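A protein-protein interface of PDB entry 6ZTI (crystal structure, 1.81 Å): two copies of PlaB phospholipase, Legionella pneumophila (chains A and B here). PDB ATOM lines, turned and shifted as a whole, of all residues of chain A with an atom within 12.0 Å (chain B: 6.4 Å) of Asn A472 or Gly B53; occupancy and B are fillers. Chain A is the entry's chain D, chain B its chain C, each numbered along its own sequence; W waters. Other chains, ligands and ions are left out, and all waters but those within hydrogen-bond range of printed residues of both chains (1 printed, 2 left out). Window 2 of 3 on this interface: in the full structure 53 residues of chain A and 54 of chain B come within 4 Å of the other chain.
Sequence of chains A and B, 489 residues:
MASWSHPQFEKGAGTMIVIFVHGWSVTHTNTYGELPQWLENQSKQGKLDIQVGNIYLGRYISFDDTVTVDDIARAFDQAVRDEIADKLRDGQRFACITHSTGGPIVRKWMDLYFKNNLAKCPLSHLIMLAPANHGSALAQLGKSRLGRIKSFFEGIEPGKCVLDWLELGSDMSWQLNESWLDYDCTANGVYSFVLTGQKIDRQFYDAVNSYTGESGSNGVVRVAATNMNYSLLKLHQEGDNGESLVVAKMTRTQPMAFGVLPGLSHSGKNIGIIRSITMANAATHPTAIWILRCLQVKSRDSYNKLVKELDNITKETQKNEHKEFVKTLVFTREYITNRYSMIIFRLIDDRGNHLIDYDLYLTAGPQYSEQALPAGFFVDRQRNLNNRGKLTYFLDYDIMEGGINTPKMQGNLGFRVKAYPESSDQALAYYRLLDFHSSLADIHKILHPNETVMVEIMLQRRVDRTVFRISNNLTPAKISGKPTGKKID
O of Gly B53 lies within hydrogen-bond range of ND2 of Asn A472 (3.0 Å).
The backbone carbonyl oxygen (O) of Ser A471 is in hydrogen-bond range of the backbone NH (N) of Leu B57.
N of Asn A473 is in hydrogen-bond range of OG of Ser A471.
The backbone NH (N) of Thr A475 sits at hydrogen-bond distance from the side-chain amide oxygen (OD1) of Asn A473, 3.1 Å away.
The side-chain amino group of Lys B87 sits at hydrogen-bond distance from the side-chain hydroxyl of Tyr B56.
Arg A469 touches Leu B57.
Ile A470 touches Leu B57 (CA to O, 3.3 Å).
Ile A470 touches Glu B83.
Ser A471 touches Tyr B56 (O to CA, 3.4 Å).
Asn A472 touches Ile B55 (CA to O, 3.4 Å).
Asn A472 touches Tyr B56.
Leu B57 touches Asn A473 (CD1 to O, 3.6 Å).
OE2 of Glu B40 touches CD1 of Leu A474, at 3.8 Å.
CD2 of Leu A474 touches O of Ile B55, 3.3 Å away.
Leu B57 touches Leu A474 (CD1 to O, 3.97 Å).
Of the printed residues of chain B, Ile A470 touches Leu B57 (3.3 Å) and Glu B83 (3.5 Å).
Asn A472 touches just these residues of chain B: Gly B53 (3.0 Å), Ile B55 (3.4 Å) and Tyr B56 (3.4 Å).
Printed residues of chain B within 4 Å of Asn A473: Leu B57.
Of the printed residues of chain B, Leu A474 touches Glu B40, Ile B55 and Leu B57.
No residue of chain A comes within 4 Å of Val B52.
Of the printed residues of chain A, Gly B53 touches Asn A472.
Printed residues of chain A within 4 Å of Glu B83: Ile A470 (3.5 Å).
The nearest residue of chain B that does not touch Asn A472 is Lys B87 (4.7 Å).
The nearest residue of chain A that does not touch Gly B53 is Leu A474 (6.8 Å).
Of the 10 printed residues of chain A, 6 touch a printed residue of chain B.
Hydrophobic or aromatic side chains of chain A within 4 Å of the printed part of chain B: Ile A470 and Leu A474.
Along chain A the printed residues that touch a printed residue of chain B span positions 469 to 474.
Among the printed residues, no Asp or Glu carboxylate lies within 4 Å of a Lys or Arg side-chain nitrogen of the other chain.
No position is printed for both chains.
Of the 12 pairs that touch across the chains among the printed residues, none has its exchanged pair printed and touching as well.
Water W1 lies within hydrogen-bond range of the side-chain amino group (NZ) of Lys B87 (2.8 Å) and the side-chain amide nitrogen (ND2) of Asn A472 (3.2 Å).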
ATOM      1  N   PHE A 468     -15.359  31.606 -38.873  1.00  0.00           N
ATOM      2  CA  PHE A 468     -15.676  30.594 -37.868  1.00  0.00           C
ATOM      3  C   PHE A 468     -14.749  30.769 -36.678  1.00  0.00           C
ATOM      4  O   PHE A 468     -13.522  30.697 -36.829  1.00  0.00           O
ATOM      5  CB  PHE A 468     -15.546  29.190 -38.440  1.00  0.00           C
ATOM      6  CG  PHE A 468     -16.420  28.171 -37.745  1.00  0.00           C
ATOM      7  CD1 PHE A 468     -16.423  28.063 -36.376  1.00  0.00           C
ATOM      8  CD2 PHE A 468     -17.239  27.331 -38.478  1.00  0.00           C
ATOM      9  CE1 PHE A 468     -17.231  27.126 -35.733  1.00  0.00           C
ATOM     10  CE2 PHE A 468     -18.044  26.396 -37.853  1.00  0.00           C
ATOM     11  CZ  PHE A 468     -18.049  26.298 -36.478  1.00  0.00           C
ATOM     12  N   ARG A 469     -15.340  30.994 -35.504  1.00  0.00           N
ATOM     13  CA  ARG A 469     -14.640  31.022 -34.231  1.00  0.00           C
ATOM     14  C   ARG A 469     -15.350  30.093 -33.254  1.00  0.00           C
ATOM     15  O   ARG A 469     -16.553  29.842 -33.371  1.00  0.00           O
ATOM     16  CB  ARG A 469     -14.590  32.435 -33.638  1.00  0.00           C
ATOM     17  CG  ARG A 469     -13.882  33.472 -34.523  1.00  0.00           C
ATOM     18  CD  ARG A 469     -12.352  33.431 -34.387  1.00  0.00           C
ATOM     19  NE  ARG A 469     -11.735  32.393 -35.225  1.00  0.00           N
ATOM     20  CZ  ARG A 469     -10.449  32.050 -35.176  1.00  0.00           C
ATOM     21  NH1 ARG A 469      -9.630  32.654 -34.322  1.00  0.00           N
ATOM     22  NH2 ARG A 469      -9.979  31.098 -35.981  1.00  0.00           N
ATOM     23  N   ILE A 470     -14.590  29.555 -32.310  1.00  0.00           N
ATOM     24  CA  ILE A 470     -15.166  28.843 -31.178  1.00  0.00           C
ATOM     25  C   ILE A 470     -14.693  29.534 -29.906  1.00  0.00           C
ATOM     26  O   ILE A 470     -13.585  30.078 -29.839  1.00  0.00           O
ATOM     27  CB  ILE A 470     -14.816  27.340 -31.153  1.00  0.00           C
ATOM     28  CG1 ILE A 470     -13.316  27.117 -30.997  1.00  0.00           C
ATOM     29  CG2 ILE A 470     -15.304  26.648 -32.421  1.00  0.00           C
ATOM     30  CD1 ILE A 470     -12.950  25.650 -30.866  1.00  0.00           C
ATOM     31  N   SER A 471     -15.553  29.527 -28.899  1.00  0.00           N
ATOM     32  CA  SER A 471     -15.239  30.147 -27.618  1.00  0.00           C
ATOM     33  C   SER A 471     -15.880  29.345 -26.502  1.00  0.00           C
ATOM     34  O   SER A 471     -17.030  28.921 -26.630  1.00  0.00           O
ATOM     35  CB  SER A 471     -15.738  31.588 -27.573  1.00  0.00           C
ATOM     36  OG  SER A 471     -15.995  31.990 -26.243  1.00  0.00           O
ATOM     37  N   ASN A 472     -15.140  29.126 -25.413  1.00  0.00           N
ATOM     38  CA  ASN A 472     -15.722  28.471 -24.247  1.00  0.00           C
ATOM     39  C   ASN A 472     -16.363  29.460 -23.269  1.00  0.00           C
ATOM     40  O   ASN A 472     -16.602  29.107 -22.109  1.00  0.00           O
ATOM     41  CB  ASN A 472     -14.686  27.600 -23.533  1.00  0.00           C
ATOM     42  CG  ASN A 472     -13.454  28.368 -23.091  1.00  0.00           C
ATOM     43  OD1 ASN A 472     -13.368  29.592 -23.234  1.00  0.00           O
ATOM     44  ND2 ASN A 472     -12.488  27.642 -22.542  1.00  0.00           N
ATOM     45  N   ASN A 473     -16.675  30.675 -23.718  1.00  0.00           N
ATOM     46  CA  ASN A 473     -17.574  31.556 -22.979  1.00  0.00           C
ATOM     47  C   ASN A 473     -19.005  31.119 -23.281  1.00  0.00           C
ATOM     48  O   ASN A 473     -19.485  31.288 -24.407  1.00  0.00           O
ATOM     49  CB  ASN A 473     -17.352  33.012 -23.376  1.00  0.00           C
ATOM     50  CG  ASN A 473     -18.083  33.983 -22.463  1.00  0.00           C
ATOM     51  OD1 ASN A 473     -18.965  33.590 -21.710  1.00  0.00           O
ATOM     52  ND2 ASN A 473     -17.724  35.258 -22.538  1.00  0.00           N
ATOM     53  N   LEU A 474     -19.692  30.548 -22.293  1.00  0.00           N
ATOM     54  CA  LEU A 474     -21.025  30.008 -22.541  1.00  0.00           C
ATOM     55  C   LEU A 474     -22.121  31.065 -22.461  1.00  0.00           C
ATOM     56  O   LEU A 474     -23.293  30.737 -22.682  1.00  0.00           O
ATOM     57  CB  LEU A 474     -21.325  28.873 -21.554  1.00  0.00           C
ATOM     58  CG  LEU A 474     -20.362  27.681 -21.592  1.00  0.00           C
ATOM     59  CD1 LEU A 474     -20.943  26.520 -20.780  1.00  0.00           C
ATOM     60  CD2 LEU A 474     -20.049  27.240 -23.032  1.00  0.00           C
ATOM     61  N   THR A 475     -21.780  32.305 -22.153  1.00  0.00           N
ATOM     62  CA  THR A 475     -22.762  33.384 -22.151  1.00  0.00           C
ATOM     63  C   THR A 475     -23.157  33.724 -23.581  1.00  0.00           C
ATOM     64  O   THR A 475     -22.306  34.190 -24.352  1.00  0.00           O
ATOM     65  CB  THR A 475     -22.191  34.611 -21.457  1.00  0.00           C
ATOM     66  OG1 THR A 475     -21.939  34.292 -20.087  1.00  0.00           O
ATOM     67  CG2 THR A 475     -23.164  35.773 -21.541  1.00  0.00           C
ATOM     68  N   PRO A 476     -24.415  33.515 -23.981  1.00  0.00           N
ATOM     69  CA  PRO A 476     -24.784  33.762 -25.378  1.00  0.00           C
ATOM     70  C   PRO A 476     -24.575  35.221 -25.753  1.00  0.00           C
ATOM     71  O   PRO A 476     -24.725  36.127 -24.928  1.00  0.00           O
ATOM     72  CB  PRO A 476     -26.270  33.374 -25.431  1.00  0.00           C
ATOM     73  CG  PRO A 476     -26.541  32.608 -24.196  1.00  0.00           C
ATOM     74  CD  PRO A 476     -25.575  33.093 -23.174  1.00  0.00           C
ATOM     75  N   ALA A 477     -24.222  35.445 -27.016  1.00  0.00           N
ATOM     76  CA  ALA A 477     -23.973  36.798 -27.494  1.00  0.00           C
ATOM     77  C   ALA A 477     -24.203  36.883 -28.994  1.00  0.00           C
ATOM     78  O   ALA A 477     -24.182  35.876 -29.708  1.00  0.00           O
ATOM     79  CB  ALA A 477     -22.545  37.245 -27.163  1.00  0.00           C
ATOM     80  N   GLU B  40     -22.864  21.231 -19.112  1.00  0.00           N
ATOM     81  CA  GLU B  40     -21.859  21.542 -18.107  1.00  0.00           C
ATOM     82  C   GLU B  40     -22.290  21.034 -16.732  1.00  0.00           C
ATOM     83  O   GLU B  40     -21.461  20.538 -15.959  1.00  0.00           O
ATOM     84  CB  GLU B  40     -21.603  23.050 -18.072  1.00  0.00           C
ATOM     85  CG  GLU B  40     -20.463  23.460 -17.148  1.00  0.00           C
ATOM     86  CD  GLU B  40     -20.272  24.964 -17.083  1.00  0.00           C
ATOM     87  OE1 GLU B  40     -21.191  25.665 -16.606  1.00  0.00           O
ATOM     88  OE2 GLU B  40     -19.206  25.448 -17.520  1.00  0.00           O
ATOM     89  N   ILE B  50     -16.615  15.860 -18.970  1.00  0.00           N
ATOM     90  CA  ILE B  50     -16.252  17.116 -19.612  1.00  0.00           C
ATOM     91  C   ILE B  50     -15.706  18.054 -18.553  1.00  0.00           C
ATOM     92  O   ILE B  50     -16.442  18.477 -17.653  1.00  0.00           O
ATOM     93  CB  ILE B  50     -17.441  17.774 -20.323  1.00  0.00           C
ATOM     94  CG1 ILE B  50     -18.135  16.782 -21.251  1.00  0.00           C
ATOM     95  CG2 ILE B  50     -16.949  18.998 -21.095  1.00  0.00           C
ATOM     96  CD1 ILE B  50     -19.454  17.273 -21.742  1.00  0.00           C
ATOM     97  N   GLN B  51     -14.435  18.414 -18.680  1.00  0.00           N
ATOM     98  CA  GLN B  51     -13.860  19.372 -17.749  1.00  0.00           C
ATOM     99  C   GLN B  51     -14.511  20.740 -17.940  1.00  0.00           C
ATOM    100  O   GLN B  51     -14.963  21.099 -19.037  1.00  0.00           O
ATOM    101  CB  GLN B  51     -12.346  19.462 -17.947  1.00  0.00           C
ATOM    102  CG  GLN B  51     -11.620  20.360 -16.935  1.00  0.00           C
ATOM    103  CD  GLN B  51     -11.722  19.850 -15.510  1.00  0.00           C
ATOM    104  OE1 GLN B  51     -12.734  20.054 -14.837  1.00  0.00           O
ATOM    105  NE2 GLN B  51     -10.667  19.182 -15.040  1.00  0.00           N
ATOM    106  N   VAL B  52     -14.591  21.491 -16.837  1.00  0.00           N
ATOM    107  CA  VAL B  52     -15.051  22.870 -16.906  1.00  0.00           C
ATOM    108  C   VAL B  52     -14.176  23.620 -17.893  1.00  0.00           C
ATOM    109  O   VAL B  52     -12.945  23.585 -17.798  1.00  0.00           O
ATOM    110  CB  VAL B  52     -15.002  23.526 -15.516  1.00  0.00           C
ATOM    111  CG1 VAL B  52     -15.411  24.988 -15.614  1.00  0.00           C
ATOM    112  CG2 VAL B  52     -15.899  22.785 -14.530  1.00  0.00           C
ATOM    113  N   GLY B  53     -14.804  24.306 -18.845  1.00  0.00           N
ATOM    114  CA  GLY B  53     -14.075  25.015 -19.871  1.00  0.00           C
ATOM    115  C   GLY B  53     -13.843  24.225 -21.138  1.00  0.00           C
ATOM    116  O   GLY B  53     -13.209  24.741 -22.068  1.00  0.00           O
ATOM    117  N   ASN B  54     -14.334  22.990 -21.213  1.00  0.00           N
ATOM    118  CA  ASN B  54     -14.194  22.183 -22.418  1.00  0.00           C
ATOM    119  C   ASN B  54     -15.500  22.074 -23.207  1.00  0.00           C
ATOM    120  O   ASN B  54     -15.642  21.177 -24.045  1.00  0.00           O
ATOM    121  CB  ASN B  54     -13.645  20.800 -22.058  1.00  0.00           C
ATOM    122  CG  ASN B  54     -12.117  20.764 -22.050  1.00  0.00           C
ATOM    123  OD1 ASN B  54     -11.453  21.735 -22.428  1.00  0.00           O
ATOM    124  ND2 ASN B  54     -11.556  19.637 -21.638  1.00  0.00           N
ATOM    125  N   ILE B  55     -16.445  22.986 -22.970  1.00  0.00           N
ATOM    126  CA  ILE B  55     -17.642  23.141 -23.797  1.00  0.00           C
ATOM    127  C   ILE B  55     -17.508  24.449 -24.568  1.00  0.00           C
ATOM    128  O   ILE B  55     -17.339  25.521 -23.972  1.00  0.00           O
ATOM    129  CB  ILE B  55     -18.927  23.120 -22.958  1.00  0.00           C
ATOM    130  CG1 ILE B  55     -18.999  21.808 -22.176  1.00  0.00           C
ATOM    131  CG2 ILE B  55     -20.182  23.283 -23.856  1.00  0.00           C
ATOM    132  CD1 ILE B  55     -20.186  21.723 -21.226  1.00  0.00           C
ATOM    133  N   TYR B  56     -17.572  24.363 -25.891  1.00  0.00           N
ATOM    134  CA  TYR B  56     -17.318  25.506 -26.753  1.00  0.00           C
ATOM    135  C   TYR B  56     -18.541  25.846 -27.589  1.00  0.00           C
ATOM    136  O   TYR B  56     -19.247  24.959 -28.083  1.00  0.00           O
ATOM    137  CB  TYR B  56     -16.125  25.244 -27.671  1.00  0.00           C
ATOM    138  CG  TYR B  56     -14.791  25.256 -26.961  1.00  0.00           C
ATOM    139  CD1 TYR B  56     -14.375  24.168 -26.211  1.00  0.00           C
ATOM    140  CD2 TYR B  56     -13.945  26.352 -27.050  1.00  0.00           C
ATOM    141  CE1 TYR B  56     -13.163  24.171 -25.566  1.00  0.00           C
ATOM    142  CE2 TYR B  56     -12.720  26.364 -26.406  1.00  0.00           C
ATOM    143  CZ  TYR B  56     -12.335  25.268 -25.664  1.00  0.00           C
ATOM    144  OH  TYR B  56     -11.124  25.248 -25.021  1.00  0.00           O
ATOM    145  N   LEU B  57     -18.783  27.141 -27.740  1.00  0.00           N
ATOM    146  CA  LEU B  57     -19.817  27.649 -28.624  1.00  0.00           C
ATOM    147  C   LEU B  57     -19.170  28.024 -29.952  1.00  0.00           C
ATOM    148  O   LEU B  57     -18.289  28.888 -30.004  1.00  0.00           O
ATOM    149  CB  LEU B  57     -20.533  28.847 -28.005  1.00  0.00           C
ATOM    150  CG  LEU B  57     -21.185  28.652 -26.636  1.00  0.00           C
ATOM    151  CD1 LEU B  57     -22.111  29.821 -26.361  1.00  0.00           C
ATOM    152  CD2 LEU B  57     -21.934  27.326 -26.566  1.00  0.00           C
ATOM    153  N   GLU B  83      -7.812  27.323 -30.984  1.00  0.00           N
ATOM    154  CA  GLU B  83      -8.330  27.344 -29.620  1.00  0.00           C
ATOM    155  C   GLU B  83      -8.019  26.103 -28.799  1.00  0.00           C
ATOM    156  O   GLU B  83      -7.823  26.229 -27.587  1.00  0.00           O
ATOM    157  CB  GLU B  83      -9.850  27.543 -29.629  1.00  0.00           C
ATOM    158  CG  GLU B  83     -10.291  28.977 -29.866  1.00  0.00           C
ATOM    159  CD  GLU B  83     -10.066  29.880 -28.657  1.00  0.00           C
ATOM    160  OE1 GLU B  83      -9.643  29.379 -27.589  1.00  0.00           O
ATOM    161  OE2 GLU B  83     -10.318  31.097 -28.777  1.00  0.00           O
ATOM    162  N   LYS B  87      -5.046  20.922 -26.544  1.00  0.00           N
ATOM    163  CA  LYS B  87      -5.844  19.872 -25.921  1.00  0.00           C
ATOM    164  C   LYS B  87      -5.947  18.644 -26.814  1.00  0.00           C
ATOM    165  O   LYS B  87      -6.038  17.518 -26.311  1.00  0.00           O
ATOM    166  CB  LYS B  87      -7.242  20.400 -25.582  1.00  0.00           C
ATOM    167  CG  LYS B  87      -7.252  21.455 -24.496  1.00  0.00           C
ATOM    168  CD  LYS B  87      -8.628  22.064 -24.344  1.00  0.00           C
ATOM    169  CE  LYS B  87      -8.684  23.050 -23.183  1.00  0.00           C
ATOM    170  NZ  LYS B  87     -10.012  23.741 -23.115  1.00  0.00           N
HETATM  171  O   HOH W   1      -9.931  26.025 -21.450  1.00  0.00           O
